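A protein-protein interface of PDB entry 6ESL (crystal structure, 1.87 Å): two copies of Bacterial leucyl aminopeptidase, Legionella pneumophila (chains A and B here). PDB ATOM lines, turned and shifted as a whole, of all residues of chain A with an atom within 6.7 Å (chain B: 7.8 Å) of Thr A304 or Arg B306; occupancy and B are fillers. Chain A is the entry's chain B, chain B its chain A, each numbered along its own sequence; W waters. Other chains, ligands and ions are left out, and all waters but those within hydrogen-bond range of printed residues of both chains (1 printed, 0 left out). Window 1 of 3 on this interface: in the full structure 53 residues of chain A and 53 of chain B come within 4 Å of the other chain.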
ATOM      1  N   VAL A 299       9.290   5.355 -34.873  1.00  0.00           N
ATOM      2  CA  VAL A 299      10.405   6.115 -34.399  1.00  0.00           C
ATOM      3  C   VAL A 299      11.494   5.124 -34.083  1.00  0.00           C
ATOM      4  O   VAL A 299      11.279   4.179 -33.241  1.00  0.00           O
ATOM      5  CB  VAL A 299       9.985   6.981 -33.164  1.00  0.00           C
ATOM      6  CG1 VAL A 299      11.154   7.720 -32.534  1.00  0.00           C
ATOM      7  CG2 VAL A 299       9.009   8.059 -33.590  1.00  0.00           C
ATOM      8  N   PHE A 300      12.664   5.305 -34.699  1.00  0.00           N
ATOM      9  CA  PHE A 300      13.801   4.439 -34.521  1.00  0.00           C
ATOM     10  C   PHE A 300      14.628   4.859 -33.300  1.00  0.00           C
ATOM     11  O   PHE A 300      14.932   5.990 -33.091  1.00  0.00           O
ATOM     12  CB  PHE A 300      14.636   4.228 -35.785  1.00  0.00           C
ATOM     13  CG  PHE A 300      14.014   3.230 -36.679  1.00  0.00           C
ATOM     14  CD1 PHE A 300      12.775   3.512 -37.294  1.00  0.00           C
ATOM     15  CD2 PHE A 300      14.441   1.919 -36.711  1.00  0.00           C
ATOM     16  CE1 PHE A 300      12.055   2.528 -38.015  1.00  0.00           C
ATOM     17  CE2 PHE A 300      13.726   0.916 -37.432  1.00  0.00           C
ATOM     18  CZ  PHE A 300      12.586   1.247 -38.142  1.00  0.00           C
ATOM     19  N   THR A 301      14.816   3.881 -32.424  1.00  0.00           N
ATOM     20  CA  THR A 301      15.498   4.089 -31.157  1.00  0.00           C
ATOM     21  C   THR A 301      17.000   3.794 -31.102  1.00  0.00           C
ATOM     22  O   THR A 301      17.633   4.051 -30.076  1.00  0.00           O
ATOM     23  CB  THR A 301      14.759   3.325 -30.045  1.00  0.00           C
ATOM     24  OG1 THR A 301      14.882   1.918 -30.275  1.00  0.00           O
ATOM     25  CG2 THR A 301      13.279   3.697 -30.060  1.00  0.00           C
ATOM     26  N   ASP A 302      17.573   3.261 -32.182  1.00  0.00           N
ATOM     27  CA  ASP A 302      19.018   2.995 -32.197  1.00  0.00           C
ATOM     28  C   ASP A 302      19.694   4.118 -33.024  1.00  0.00           C
ATOM     29  O   ASP A 302      19.189   4.521 -34.081  1.00  0.00           O
ATOM     30  CB  ASP A 302      19.434   1.574 -32.502  1.00  0.00           C
ATOM     31  CG  ASP A 302      19.159   1.186 -33.897  1.00  0.00           C
ATOM     32  OD1 ASP A 302      18.386   1.896 -34.571  1.00  0.00           O
ATOM     33  OD2 ASP A 302      19.721   0.159 -34.315  1.00  0.00           O
ATOM     34  N   TYR A 303      20.819   4.614 -32.491  1.00  0.00           N
ATOM     35  CA  TYR A 303      21.655   5.691 -33.059  1.00  0.00           C
ATOM     36  C   TYR A 303      20.942   7.020 -33.185  1.00  0.00           C
ATOM     37  O   TYR A 303      21.198   7.807 -34.099  1.00  0.00           O
ATOM     38  CB  TYR A 303      22.303   5.240 -34.371  1.00  0.00           C
ATOM     39  CG  TYR A 303      23.023   3.934 -34.117  1.00  0.00           C
ATOM     40  CD1 TYR A 303      24.305   3.902 -33.549  1.00  0.00           C
ATOM     41  CD2 TYR A 303      22.427   2.694 -34.395  1.00  0.00           C
ATOM     42  CE1 TYR A 303      24.935   2.709 -33.296  1.00  0.00           C
ATOM     43  CE2 TYR A 303      23.102   1.513 -34.162  1.00  0.00           C
ATOM     44  CZ  TYR A 303      24.336   1.521 -33.587  1.00  0.00           C
ATOM     45  OH  TYR A 303      24.955   0.310 -33.378  1.00  0.00           O
ATOM     46  N   THR A 304      20.080   7.284 -32.212  1.00  0.00           N
ATOM     47  CA  THR A 304      19.294   8.496 -32.232  1.00  0.00           C
ATOM     48  C   THR A 304      19.232   9.086 -30.779  1.00  0.00           C
ATOM     49  O   THR A 304      19.387   8.365 -29.831  1.00  0.00           O
ATOM     50  CB  THR A 304      17.846   8.243 -32.636  1.00  0.00           C
ATOM     51  OG1 THR A 304      17.240   7.237 -31.846  1.00  0.00           O
ATOM     52  CG2 THR A 304      17.722   7.822 -34.156  1.00  0.00           C
ATOM     53  N   ASP A 305      18.914  10.352 -30.700  1.00  0.00           N
ATOM     54  CA  ASP A 305      18.780  11.091 -29.468  1.00  0.00           C
ATOM     55  C   ASP A 305      17.458  10.759 -28.868  1.00  0.00           C
ATOM     56  O   ASP A 305      16.418  10.893 -29.480  1.00  0.00           O
ATOM     57  CB  ASP A 305      18.889  12.580 -29.703  1.00  0.00           C
ATOM     58  CG  ASP A 305      18.793  13.394 -28.424  1.00  0.00           C
ATOM     59  OD1 ASP A 305      19.780  13.354 -27.682  1.00  0.00           O
ATOM     60  OD2 ASP A 305      17.714  14.055 -28.155  1.00  0.00           O
ATOM     61  N   ARG A 306      17.517  10.340 -27.615  1.00  0.00           N
ATOM     62  CA  ARG A 306      16.331   9.973 -26.880  1.00  0.00           C
ATOM     63  C   ARG A 306      15.309  11.071 -26.723  1.00  0.00           C
ATOM     64  O   ARG A 306      14.117  10.855 -27.042  1.00  0.00           O
ATOM     65  CB  ARG A 306      16.771   9.378 -25.509  1.00  0.00           C
ATOM     66  CG  ARG A 306      15.606   9.188 -24.525  1.00  0.00           C
ATOM     67  CD  ARG A 306      16.068   8.484 -23.278  1.00  0.00           C
ATOM     68  NE  ARG A 306      14.909   7.800 -22.664  1.00  0.00           N
ATOM     69  CZ  ARG A 306      14.999   7.012 -21.579  1.00  0.00           C
ATOM     70  NH1 ARG A 306      16.191   6.762 -20.998  1.00  0.00           N
ATOM     71  NH2 ARG A 306      13.900   6.504 -21.048  1.00  0.00           N
ATOM     72  N   ASP A 307      15.687  12.259 -26.255  1.00  0.00           N
ATOM     73  CA  ASP A 307      14.723  13.341 -26.137  1.00  0.00           C
ATOM     74  C   ASP A 307      14.159  13.804 -27.472  1.00  0.00           C
ATOM     75  O   ASP A 307      13.000  14.079 -27.593  1.00  0.00           O
ATOM     76  CB  ASP A 307      15.281  14.546 -25.376  1.00  0.00           C
ATOM     77  CG  ASP A 307      15.488  14.270 -23.901  1.00  0.00           C
ATOM     78  OD1 ASP A 307      14.958  13.270 -23.370  1.00  0.00           O
ATOM     79  OD2 ASP A 307      16.192  15.074 -23.263  1.00  0.00           O
ATOM     80  N   LEU A 308      15.009  13.895 -28.509  1.00  0.00           N
ATOM     81  CA  LEU A 308      14.467  14.365 -29.808  1.00  0.00           C
ATOM     82  C   LEU A 308      13.487  13.337 -30.401  1.00  0.00           C
ATOM     83  O   LEU A 308      12.468  13.707 -30.989  1.00  0.00           O
ATOM     84  CB  LEU A 308      15.623  14.670 -30.770  1.00  0.00           C
ATOM     85  CG  LEU A 308      15.194  15.345 -32.091  1.00  0.00           C
ATOM     86  CD1 LEU A 308      14.641  16.710 -31.826  1.00  0.00           C
ATOM     87  CD2 LEU A 308      16.383  15.412 -33.043  1.00  0.00           C
ATOM     88  N   SER A 309      13.774  12.058 -30.198  1.00  0.00           N
ATOM     89  CA  SER A 309      12.929  10.938 -30.658  1.00  0.00           C
ATOM     90  C   SER A 309      11.580  10.958 -29.986  1.00  0.00           C
ATOM     91  O   SER A 309      10.498  10.903 -30.653  1.00  0.00           O
ATOM     92  CB  SER A 309      13.595   9.590 -30.472  1.00  0.00           C
ATOM     93  OG  SER A 309      14.859   9.512 -31.120  1.00  0.00           O
ATOM     94  N   ASN A 310      11.604  11.150 -28.684  1.00  0.00           N
ATOM     95  CA  ASN A 310      10.332  11.372 -27.937  1.00  0.00           C
ATOM     96  C   ASN A 310       9.561  12.576 -28.422  1.00  0.00           C
ATOM     97  O   ASN A 310       8.345  12.517 -28.534  1.00  0.00           O
ATOM     98  CB  ASN A 310      10.577  11.539 -26.421  1.00  0.00           C
ATOM     99  CG  ASN A 310      11.067  10.245 -25.729  1.00  0.00           C
ATOM    100  OD1 ASN A 310      10.848   9.124 -26.225  1.00  0.00           O
ATOM    101  ND2 ASN A 310      11.643  10.411 -24.495  1.00  0.00           N
ATOM    102  N   HIS A 336      21.154   9.842 -40.185  1.00  0.00           N
ATOM    103  CA  HIS A 336      21.114  10.364 -38.829  1.00  0.00           C
ATOM    104  C   HIS A 336      22.287   9.877 -38.016  1.00  0.00           C
ATOM    105  O   HIS A 336      22.751  10.609 -37.116  1.00  0.00           O
ATOM    106  CB  HIS A 336      19.816   9.950 -38.144  1.00  0.00           C
ATOM    107  CG  HIS A 336      19.609   8.475 -38.127  1.00  0.00           C
ATOM    108  ND1 HIS A 336      19.283   7.759 -39.288  1.00  0.00           N
ATOM    109  CD2 HIS A 336      19.716   7.563 -37.108  1.00  0.00           C
ATOM    110  CE1 HIS A 336      19.225   6.458 -38.938  1.00  0.00           C
ATOM    111  NE2 HIS A 336      19.493   6.326 -37.626  1.00  0.00           N
ATOM    112  N   ALA A 337      22.827   8.710 -38.343  1.00  0.00           N
ATOM    113  CA  ALA A 337      23.914   8.140 -37.564  1.00  0.00           C
ATOM    114  C   ALA A 337      25.170   8.974 -37.611  1.00  0.00           C
ATOM    115  O   ALA A 337      25.949   9.003 -36.650  1.00  0.00           O
ATOM    116  CB  ALA A 337      24.200   6.683 -37.981  1.00  0.00           C
ATOM    117  N   ASN A 340      24.655  11.632 -35.095  1.00  0.00           N
ATOM    118  CA  ASN A 340      24.623  11.038 -33.753  1.00  0.00           C
ATOM    119  C   ASN A 340      26.051  10.724 -33.242  1.00  0.00           C
ATOM    120  O   ASN A 340      26.330  10.811 -31.999  1.00  0.00           O
ATOM    121  CB  ASN A 340      23.794   9.790 -33.737  1.00  0.00           C
ATOM    122  CG  ASN A 340      23.725   9.128 -32.365  1.00  0.00           C
ATOM    123  OD1 ASN A 340      24.277   8.065 -32.193  1.00  0.00           O
ATOM    124  ND2 ASN A 340      22.915   9.696 -31.444  1.00  0.00           N
ATOM    125  N   PRO A 345      22.122  16.010 -31.599  1.00  0.00           N
ATOM    126  CA  PRO A 345      20.838  15.342 -31.445  1.00  0.00           C
ATOM    127  C   PRO A 345      20.149  15.055 -32.817  1.00  0.00           C
ATOM    128  O   PRO A 345      20.043  15.959 -33.614  1.00  0.00           O
ATOM    129  CB  PRO A 345      20.034  16.343 -30.601  1.00  0.00           C
ATOM    130  CG  PRO A 345      21.082  17.022 -29.748  1.00  0.00           C
ATOM    131  CD  PRO A 345      22.132  17.263 -30.814  1.00  0.00           C
ATOM    132  N   ALA A 346      19.792  13.790 -33.056  1.00  0.00           N
ATOM    133  CA  ALA A 346      19.309  13.340 -34.333  1.00  0.00           C
ATOM    134  C   ALA A 346      18.255  12.295 -34.158  1.00  0.00           C
ATOM    135  O   ALA A 346      18.290  11.487 -33.198  1.00  0.00           O
ATOM    136  CB  ALA A 346      20.457  12.802 -35.179  1.00  0.00           C
ATOM    137  N   ALA A 347      17.287  12.310 -35.041  1.00  0.00           N
ATOM    138  CA  ALA A 347      16.130  11.405 -34.912  1.00  0.00           C
ATOM    139  C   ALA A 347      15.736  10.912 -36.301  1.00  0.00           C
ATOM    140  O   ALA A 347      16.047  11.590 -37.300  1.00  0.00           O
ATOM    141  CB  ALA A 347      14.968  12.111 -34.281  1.00  0.00           C
ATOM    142  N   PHE A 348      15.030   9.762 -36.305  1.00  0.00           N
ATOM    143  CA  PHE A 348      14.743   9.008 -37.514  1.00  0.00           C
ATOM    144  C   PHE A 348      13.319   8.378 -37.400  1.00  0.00           C
ATOM    145  O   PHE A 348      13.133   7.277 -36.847  1.00  0.00           O
ATOM    146  CB  PHE A 348      15.811   7.953 -37.772  1.00  0.00           C
ATOM    147  CG  PHE A 348      15.573   7.078 -38.966  1.00  0.00           C
ATOM    148  CD1 PHE A 348      14.918   7.526 -40.092  1.00  0.00           C
ATOM    149  CD2 PHE A 348      16.012   5.775 -38.980  1.00  0.00           C
ATOM    150  CE1 PHE A 348      14.659   6.634 -41.164  1.00  0.00           C
ATOM    151  CE2 PHE A 348      15.797   4.901 -40.066  1.00  0.00           C
ATOM    152  CZ  PHE A 348      15.164   5.360 -41.189  1.00  0.00           C
ATOM    153  N   TYR B 113       9.956  -5.969 -26.441  1.00  0.00           N
ATOM    154  CA  TYR B 113       8.794  -5.820 -25.607  1.00  0.00           C
ATOM    155  C   TYR B 113       7.658  -5.522 -26.568  1.00  0.00           C
ATOM    156  O   TYR B 113       7.679  -4.544 -27.261  1.00  0.00           O
ATOM    157  CB  TYR B 113       8.949  -4.635 -24.656  1.00  0.00           C
ATOM    158  CG  TYR B 113      10.217  -4.596 -23.846  1.00  0.00           C
ATOM    159  CD1 TYR B 113      10.472  -5.531 -22.888  1.00  0.00           C
ATOM    160  CD2 TYR B 113      11.136  -3.606 -24.031  1.00  0.00           C
ATOM    161  CE1 TYR B 113      11.611  -5.487 -22.143  1.00  0.00           C
ATOM    162  CE2 TYR B 113      12.276  -3.555 -23.294  1.00  0.00           C
ATOM    163  CZ  TYR B 113      12.513  -4.500 -22.364  1.00  0.00           C
ATOM    164  OH  TYR B 113      13.660  -4.441 -21.640  1.00  0.00           O
ATOM    165  N   VAL B 299       6.038   9.620 -18.455  1.00  0.00           N
ATOM    166  CA  VAL B 299       7.032   8.596 -18.507  1.00  0.00           C
ATOM    167  C   VAL B 299       8.329   9.339 -18.253  1.00  0.00           C
ATOM    168  O   VAL B 299       8.676  10.323 -18.939  1.00  0.00           O
ATOM    169  CB  VAL B 299       7.034   7.845 -19.853  1.00  0.00           C
ATOM    170  CG1 VAL B 299       8.235   6.883 -19.991  1.00  0.00           C
ATOM    171  CG2 VAL B 299       5.757   6.988 -20.009  1.00  0.00           C
ATOM    172  N   PHE B 300       9.045   8.920 -17.193  1.00  0.00           N
ATOM    173  CA  PHE B 300      10.288   9.595 -16.840  1.00  0.00           C
ATOM    174  C   PHE B 300      11.502   9.054 -17.609  1.00  0.00           C
ATOM    175  O   PHE B 300      11.653   7.889 -17.784  1.00  0.00           O
ATOM    176  CB  PHE B 300      10.482   9.639 -15.318  1.00  0.00           C
ATOM    177  CG  PHE B 300       9.710  10.767 -14.728  1.00  0.00           C
ATOM    178  CD1 PHE B 300       8.310  10.711 -14.715  1.00  0.00           C
ATOM    179  CD2 PHE B 300      10.301  11.956 -14.413  1.00  0.00           C
ATOM    180  CE1 PHE B 300       7.531  11.831 -14.280  1.00  0.00           C
ATOM    181  CE2 PHE B 300       9.547  13.049 -13.949  1.00  0.00           C
ATOM    182  CZ  PHE B 300       8.153  12.966 -13.814  1.00  0.00           C
ATOM    183  N   THR B 301      12.336   9.952 -18.072  1.00  0.00           N
ATOM    184  CA  THR B 301      13.335   9.618 -19.088  1.00  0.00           C
ATOM    185  C   THR B 301      14.754   9.637 -18.605  1.00  0.00           C
ATOM    186  O   THR B 301      15.596   9.271 -19.387  1.00  0.00           O
ATOM    187  CB  THR B 301      13.238  10.582 -20.302  1.00  0.00           C
ATOM    188  OG1 THR B 301      13.561  11.963 -19.918  1.00  0.00           O
ATOM    189  CG2 THR B 301      11.880  10.449 -20.911  1.00  0.00           C
ATOM    190  N   TYR B 303      17.575   8.083 -15.833  1.00  0.00           N
ATOM    191  CA  TYR B 303      17.857   6.880 -15.000  1.00  0.00           C
ATOM    192  C   TYR B 303      16.878   5.760 -15.268  1.00  0.00           C
ATOM    193  O   TYR B 303      16.556   4.981 -14.374  1.00  0.00           O
ATOM    194  CB  TYR B 303      17.890   7.280 -13.489  1.00  0.00           C
ATOM    195  CG  TYR B 303      18.836   8.440 -13.284  1.00  0.00           C
ATOM    196  CD1 TYR B 303      20.196   8.242 -13.222  1.00  0.00           C
ATOM    197  CD2 TYR B 303      18.363   9.734 -13.138  1.00  0.00           C
ATOM    198  CE1 TYR B 303      21.065   9.320 -13.101  1.00  0.00           C
ATOM    199  CE2 TYR B 303      19.240  10.804 -12.976  1.00  0.00           C
ATOM    200  CZ  TYR B 303      20.581  10.606 -12.990  1.00  0.00           C
ATOM    201  OH  TYR B 303      21.426  11.688 -12.805  1.00  0.00           O
ATOM    202  N   THR B 304      16.396   5.705 -16.509  1.00  0.00           N
ATOM    203  CA  THR B 304      15.509   4.674 -16.938  1.00  0.00           C
ATOM    204  C   THR B 304      15.968   4.102 -18.304  1.00  0.00           C
ATOM    205  O   THR B 304      16.672   4.765 -19.042  1.00  0.00           O
ATOM    206  CB  THR B 304      14.055   5.175 -17.127  1.00  0.00           C
ATOM    207  OG1 THR B 304      14.029   6.284 -18.020  1.00  0.00           O
ATOM    208  CG2 THR B 304      13.403   5.624 -15.806  1.00  0.00           C
ATOM    209  N   ASP B 305      15.463   2.918 -18.615  1.00  0.00           N
ATOM    210  CA  ASP B 305      15.803   2.202 -19.800  1.00  0.00           C
ATOM    211  C   ASP B 305      14.976   2.757 -20.931  1.00  0.00           C
ATOM    212  O   ASP B 305      13.745   2.846 -20.840  1.00  0.00           O
ATOM    213  CB  ASP B 305      15.479   0.734 -19.661  1.00  0.00           C
ATOM    214  CG  ASP B 305      15.862  -0.074 -20.944  1.00  0.00           C
ATOM    215  OD1 ASP B 305      17.054  -0.201 -21.190  1.00  0.00           O
ATOM    216  OD2 ASP B 305      14.957  -0.500 -21.703  1.00  0.00           O
ATOM    217  N   ARG B 306      15.644   3.160 -21.989  1.00  0.00           N
ATOM    218  CA  ARG B 306      14.957   3.721 -23.109  1.00  0.00           C
ATOM    219  C   ARG B 306      13.920   2.816 -23.805  1.00  0.00           C
ATOM    220  O   ARG B 306      12.777   3.237 -24.034  1.00  0.00           O
ATOM    221  CB  ARG B 306      16.005   4.222 -24.110  1.00  0.00           C
ATOM    222  CG  ARG B 306      15.373   4.874 -25.310  1.00  0.00           C
ATOM    223  CD  ARG B 306      16.535   5.289 -26.228  1.00  0.00           C
ATOM    224  NE  ARG B 306      15.971   5.978 -27.334  1.00  0.00           N
ATOM    225  CZ  ARG B 306      16.633   6.665 -28.268  1.00  0.00           C
ATOM    226  NH1 ARG B 306      17.947   6.815 -28.149  1.00  0.00           N
ATOM    227  NH2 ARG B 306      15.942   7.288 -29.230  1.00  0.00           N
ATOM    228  N   ASP B 307      14.255   1.587 -24.111  1.00  0.00           N
ATOM    229  CA  ASP B 307      13.252   0.711 -24.732  1.00  0.00           C
ATOM    230  C   ASP B 307      12.112   0.336 -23.792  1.00  0.00           C
ATOM    231  O   ASP B 307      10.987   0.277 -24.197  1.00  0.00           O
ATOM    232  CB  ASP B 307      13.837  -0.621 -25.269  1.00  0.00           C
ATOM    233  CG  ASP B 307      14.883  -0.405 -26.393  1.00  0.00           C
ATOM    234  OD1 ASP B 307      14.755   0.589 -27.107  1.00  0.00           O
ATOM    235  OD2 ASP B 307      15.827  -1.232 -26.477  1.00  0.00           O
ATOM    236  N   LEU B 308      12.386   0.117 -22.518  1.00  0.00           N
ATOM    237  CA  LEU B 308      11.316  -0.204 -21.589  1.00  0.00           C
ATOM    238  C   LEU B 308      10.376   0.996 -21.398  1.00  0.00           C
ATOM    239  O   LEU B 308       9.135   0.834 -21.285  1.00  0.00           O
ATOM    240  CB  LEU B 308      11.874  -0.708 -20.267  1.00  0.00           C
ATOM    241  CG  LEU B 308      10.803  -1.325 -19.331  1.00  0.00           C
ATOM    242  CD1 LEU B 308      10.147  -2.531 -19.908  1.00  0.00           C
ATOM    243  CD2 LEU B 308      11.360  -1.620 -17.946  1.00  0.00           C
ATOM    244  N   SER B 309      10.944   2.206 -21.400  1.00  0.00           N
ATOM    245  CA  SER B 309      10.166   3.448 -21.287  1.00  0.00           C
ATOM    246  C   SER B 309       9.226   3.653 -22.434  1.00  0.00           C
ATOM    247  O   SER B 309       8.035   3.944 -22.251  1.00  0.00           O
ATOM    248  CB  SER B 309      11.065   4.691 -21.137  1.00  0.00           C
ATOM    249  OG  SER B 309      11.930   4.549 -20.000  1.00  0.00           O
ATOM    250  N   ASN B 310       9.763   3.404 -23.642  1.00  0.00           N
ATOM    251  CA  ASN B 310       8.921   3.421 -24.844  1.00  0.00           C
ATOM    252  C   ASN B 310       7.821   2.405 -24.793  1.00  0.00           C
ATOM    253  O   ASN B 310       6.690   2.693 -25.205  1.00  0.00           O
ATOM    254  CB  ASN B 310       9.771   3.167 -26.125  1.00  0.00           C
ATOM    255  CG  ASN B 310      10.674   4.368 -26.489  1.00  0.00           C
ATOM    256  OD1 ASN B 310      10.347   5.537 -26.197  1.00  0.00           O
ATOM    257  ND2 ASN B 310      11.788   4.069 -27.190  1.00  0.00           N
ATOM    258  N   TYR B 311       8.113   1.234 -24.267  1.00  0.00           N
ATOM    259  CA  TYR B 311       7.090   0.245 -24.062  1.00  0.00           C
ATOM    260  C   TYR B 311       5.972   0.718 -23.103  1.00  0.00           C
ATOM    261  O   TYR B 311       4.768   0.509 -23.361  1.00  0.00           O
ATOM    262  CB  TYR B 311       7.713  -1.078 -23.546  1.00  0.00           C
ATOM    263  CG  TYR B 311       6.777  -2.182 -23.489  1.00  0.00           C
ATOM    264  CD1 TYR B 311       6.165  -2.648 -24.659  1.00  0.00           C
ATOM    265  CD2 TYR B 311       6.490  -2.849 -22.296  1.00  0.00           C
ATOM    266  CE1 TYR B 311       5.248  -3.715 -24.629  1.00  0.00           C
ATOM    267  CE2 TYR B 311       5.589  -3.896 -22.250  1.00  0.00           C
ATOM    268  CZ  TYR B 311       5.003  -4.355 -23.424  1.00  0.00           C
ATOM    269  OH  TYR B 311       4.095  -5.388 -23.385  1.00  0.00           O
ATOM    270  N   LEU B 312       6.352   1.351 -22.019  1.00  0.00           N
ATOM    271  CA  LEU B 312       5.292   1.921 -21.147  1.00  0.00           C
ATOM    272  C   LEU B 312       4.390   2.883 -21.925  1.00  0.00           C
ATOM    273  O   LEU B 312       3.201   2.875 -21.760  1.00  0.00           O
ATOM    274  CB  LEU B 312       5.861   2.658 -19.944  1.00  0.00           C
ATOM    275  CG  LEU B 312       6.527   1.866 -18.822  1.00  0.00           C
ATOM    276  CD1 LEU B 312       6.661   2.772 -17.598  1.00  0.00           C
ATOM    277  CD2 LEU B 312       5.847   0.570 -18.401  1.00  0.00           C
ATOM    278  N   ASN B 340      18.487   0.543 -12.342  1.00  0.00           N
ATOM    279  CA  ASN B 340      19.126   1.124 -13.525  1.00  0.00           C
ATOM    280  C   ASN B 340      20.665   1.162 -13.364  1.00  0.00           C
ATOM    281  O   ASN B 340      21.393   0.983 -14.362  1.00  0.00           O
ATOM    282  CB  ASN B 340      18.585   2.510 -13.779  1.00  0.00           C
ATOM    283  CG  ASN B 340      19.249   3.191 -14.987  1.00  0.00           C
ATOM    284  OD1 ASN B 340      20.008   4.128 -14.796  1.00  0.00           O
ATOM    285  ND2 ASN B 340      18.851   2.855 -16.162  1.00  0.00           N
ATOM    286  N   PRO B 345      16.972  -3.279 -16.925  1.00  0.00           N
ATOM    287  CA  PRO B 345      16.000  -2.379 -17.526  1.00  0.00           C
ATOM    288  C   PRO B 345      14.858  -1.981 -16.575  1.00  0.00           C
ATOM    289  O   PRO B 345      14.252  -2.836 -15.992  1.00  0.00           O
ATOM    290  CB  PRO B 345      15.472  -3.201 -18.733  1.00  0.00           C
ATOM    291  CG  PRO B 345      16.634  -4.082 -19.107  1.00  0.00           C
ATOM    292  CD  PRO B 345      17.100  -4.506 -17.751  1.00  0.00           C
ATOM    293  N   ALA B 346      14.677  -0.666 -16.389  1.00  0.00           N
ATOM    294  CA  ALA B 346      13.763  -0.142 -15.382  1.00  0.00           C
ATOM    295  C   ALA B 346      13.116   1.131 -15.903  1.00  0.00           C
ATOM    296  O   ALA B 346      13.736   1.903 -16.634  1.00  0.00           O
ATOM    297  CB  ALA B 346      14.497   0.120 -14.078  1.00  0.00           C
ATOM    298  N   ALA B 347      11.846   1.287 -15.594  1.00  0.00           N
ATOM    299  CA  ALA B 347      11.101   2.400 -16.102  1.00  0.00           C
ATOM    300  C   ALA B 347      10.180   2.927 -14.968  1.00  0.00           C
ATOM    301  O   ALA B 347       9.863   2.209 -14.016  1.00  0.00           O
ATOM    302  CB  ALA B 347      10.300   1.951 -17.275  1.00  0.00           C
HETATM  303  O   HOH W   1      15.651  12.858 -21.051  1.00  0.00           O
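NH1 of Arg B306 sits close to O of Thr A301, at 3.4 Å. The guanidinium group (NH2) of Arg A306 sits at hydrogen-bond distance from the side-chain hydroxyl (OG) of Ser B309 (3.0 Å). OG1 of Thr A301 is in hydrogen-bond range of OD1 of Asp B307 (3.4 Å). The backbone carbonyl oxygen (O) of Thr A304 sits at hydrogen-bond distance from the guanidinium group (NH1) of Arg B306. The guanidinium group (NH2) of Arg B306 lies within hydrogen-bond range of the side-chain hydroxyl (OG) of Ser A309, 3.1 Å away. The backbone carbonyl oxygen (O) of Thr B301 lies within hydrogen-bond range of the guanidinium group (NH1) of Arg A306. O of Thr B304 lies within hydrogen-bond range of NH1 of Arg A306 (2.8 Å).
N of Asp A307 sits at hydrogen-bond distance from OD2 of Asp A305 (3.3 Å). The backbone carbonyl oxygen (O) of Asp B305 lies within hydrogen-bond range of the side-chain hydroxyl (OG) of Ser B309. The side-chain hydroxyl of Ser A309 sits at hydrogen-bond distance from the side-chain hydroxyl of Thr A304 (3.4 Å). OG1 of Thr B304 is in hydrogen-bond range of OG of Ser B309 (3.4 Å). O of Phe B300 is in hydrogen-bond range of OG1 of Thr B304 (2.9 Å). The backbone NH of Asp B305 lies within hydrogen-bond range of the backbone carbonyl oxygen of Ala B346 (2.8 Å).
Thr A301 touches Asn B310. Asp A305 touches Arg B306 (O to NH2, 3.6 Å). O of Asp B305 touches NH2 of Arg A306, at 3.7 Å. Arg A306 touches Arg B306 (CA to NH2, 3.6 Å). OG1 of Thr B301 touches OD1 of Asp A307, at 3.9 Å. Thr B301 touches Asn A310 (CG2 to ND2, 3.6 Å). Asn B310 touches Asn A310.
Val A299 touches none of the printed residues of chain B. Of chain B, only Arg B306 comes within 4 Å of Thr A304. Of the printed residues of chain B, Asp A307 touches Thr B301. Of the printed residues of chain A, Thr B304 touches Arg A306 (2.8 Å). The nearest printed residue of chain B that does not touch Thr A304 is Asn B310 (7.8 Å). The nearest residue of chain A that does not touch Arg B306 is Phe A300 (4.2 Å).
Among the printed residues, 14 pairs touch across the chains.
Thr A301 touches Arg B306, and with the chains exchanged Arg A306 touches Thr B301. Thr A301 touches Asn B310, and with the chains exchanged Asn A310 touches Thr B301. Asp A305 touches Arg B306, and with the chains exchanged Arg A306 touches Asp B305. Arg B306 touches its own counterpart, Arg A306. Positions printed for both chains: 299, 300, 301, 303, 304, 305, 306, 307, 308, 309, 310, 340, 345, 346 and 347. Of the 14 pairs that touch across the chains among the printed residues, 14 have their exchanged pair printed and touching as well.
Water W1 lies within hydrogen-bond range of OD1 of Asp A307 (2.5 Å) and OG1 of Thr B301 (2.5 Å).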
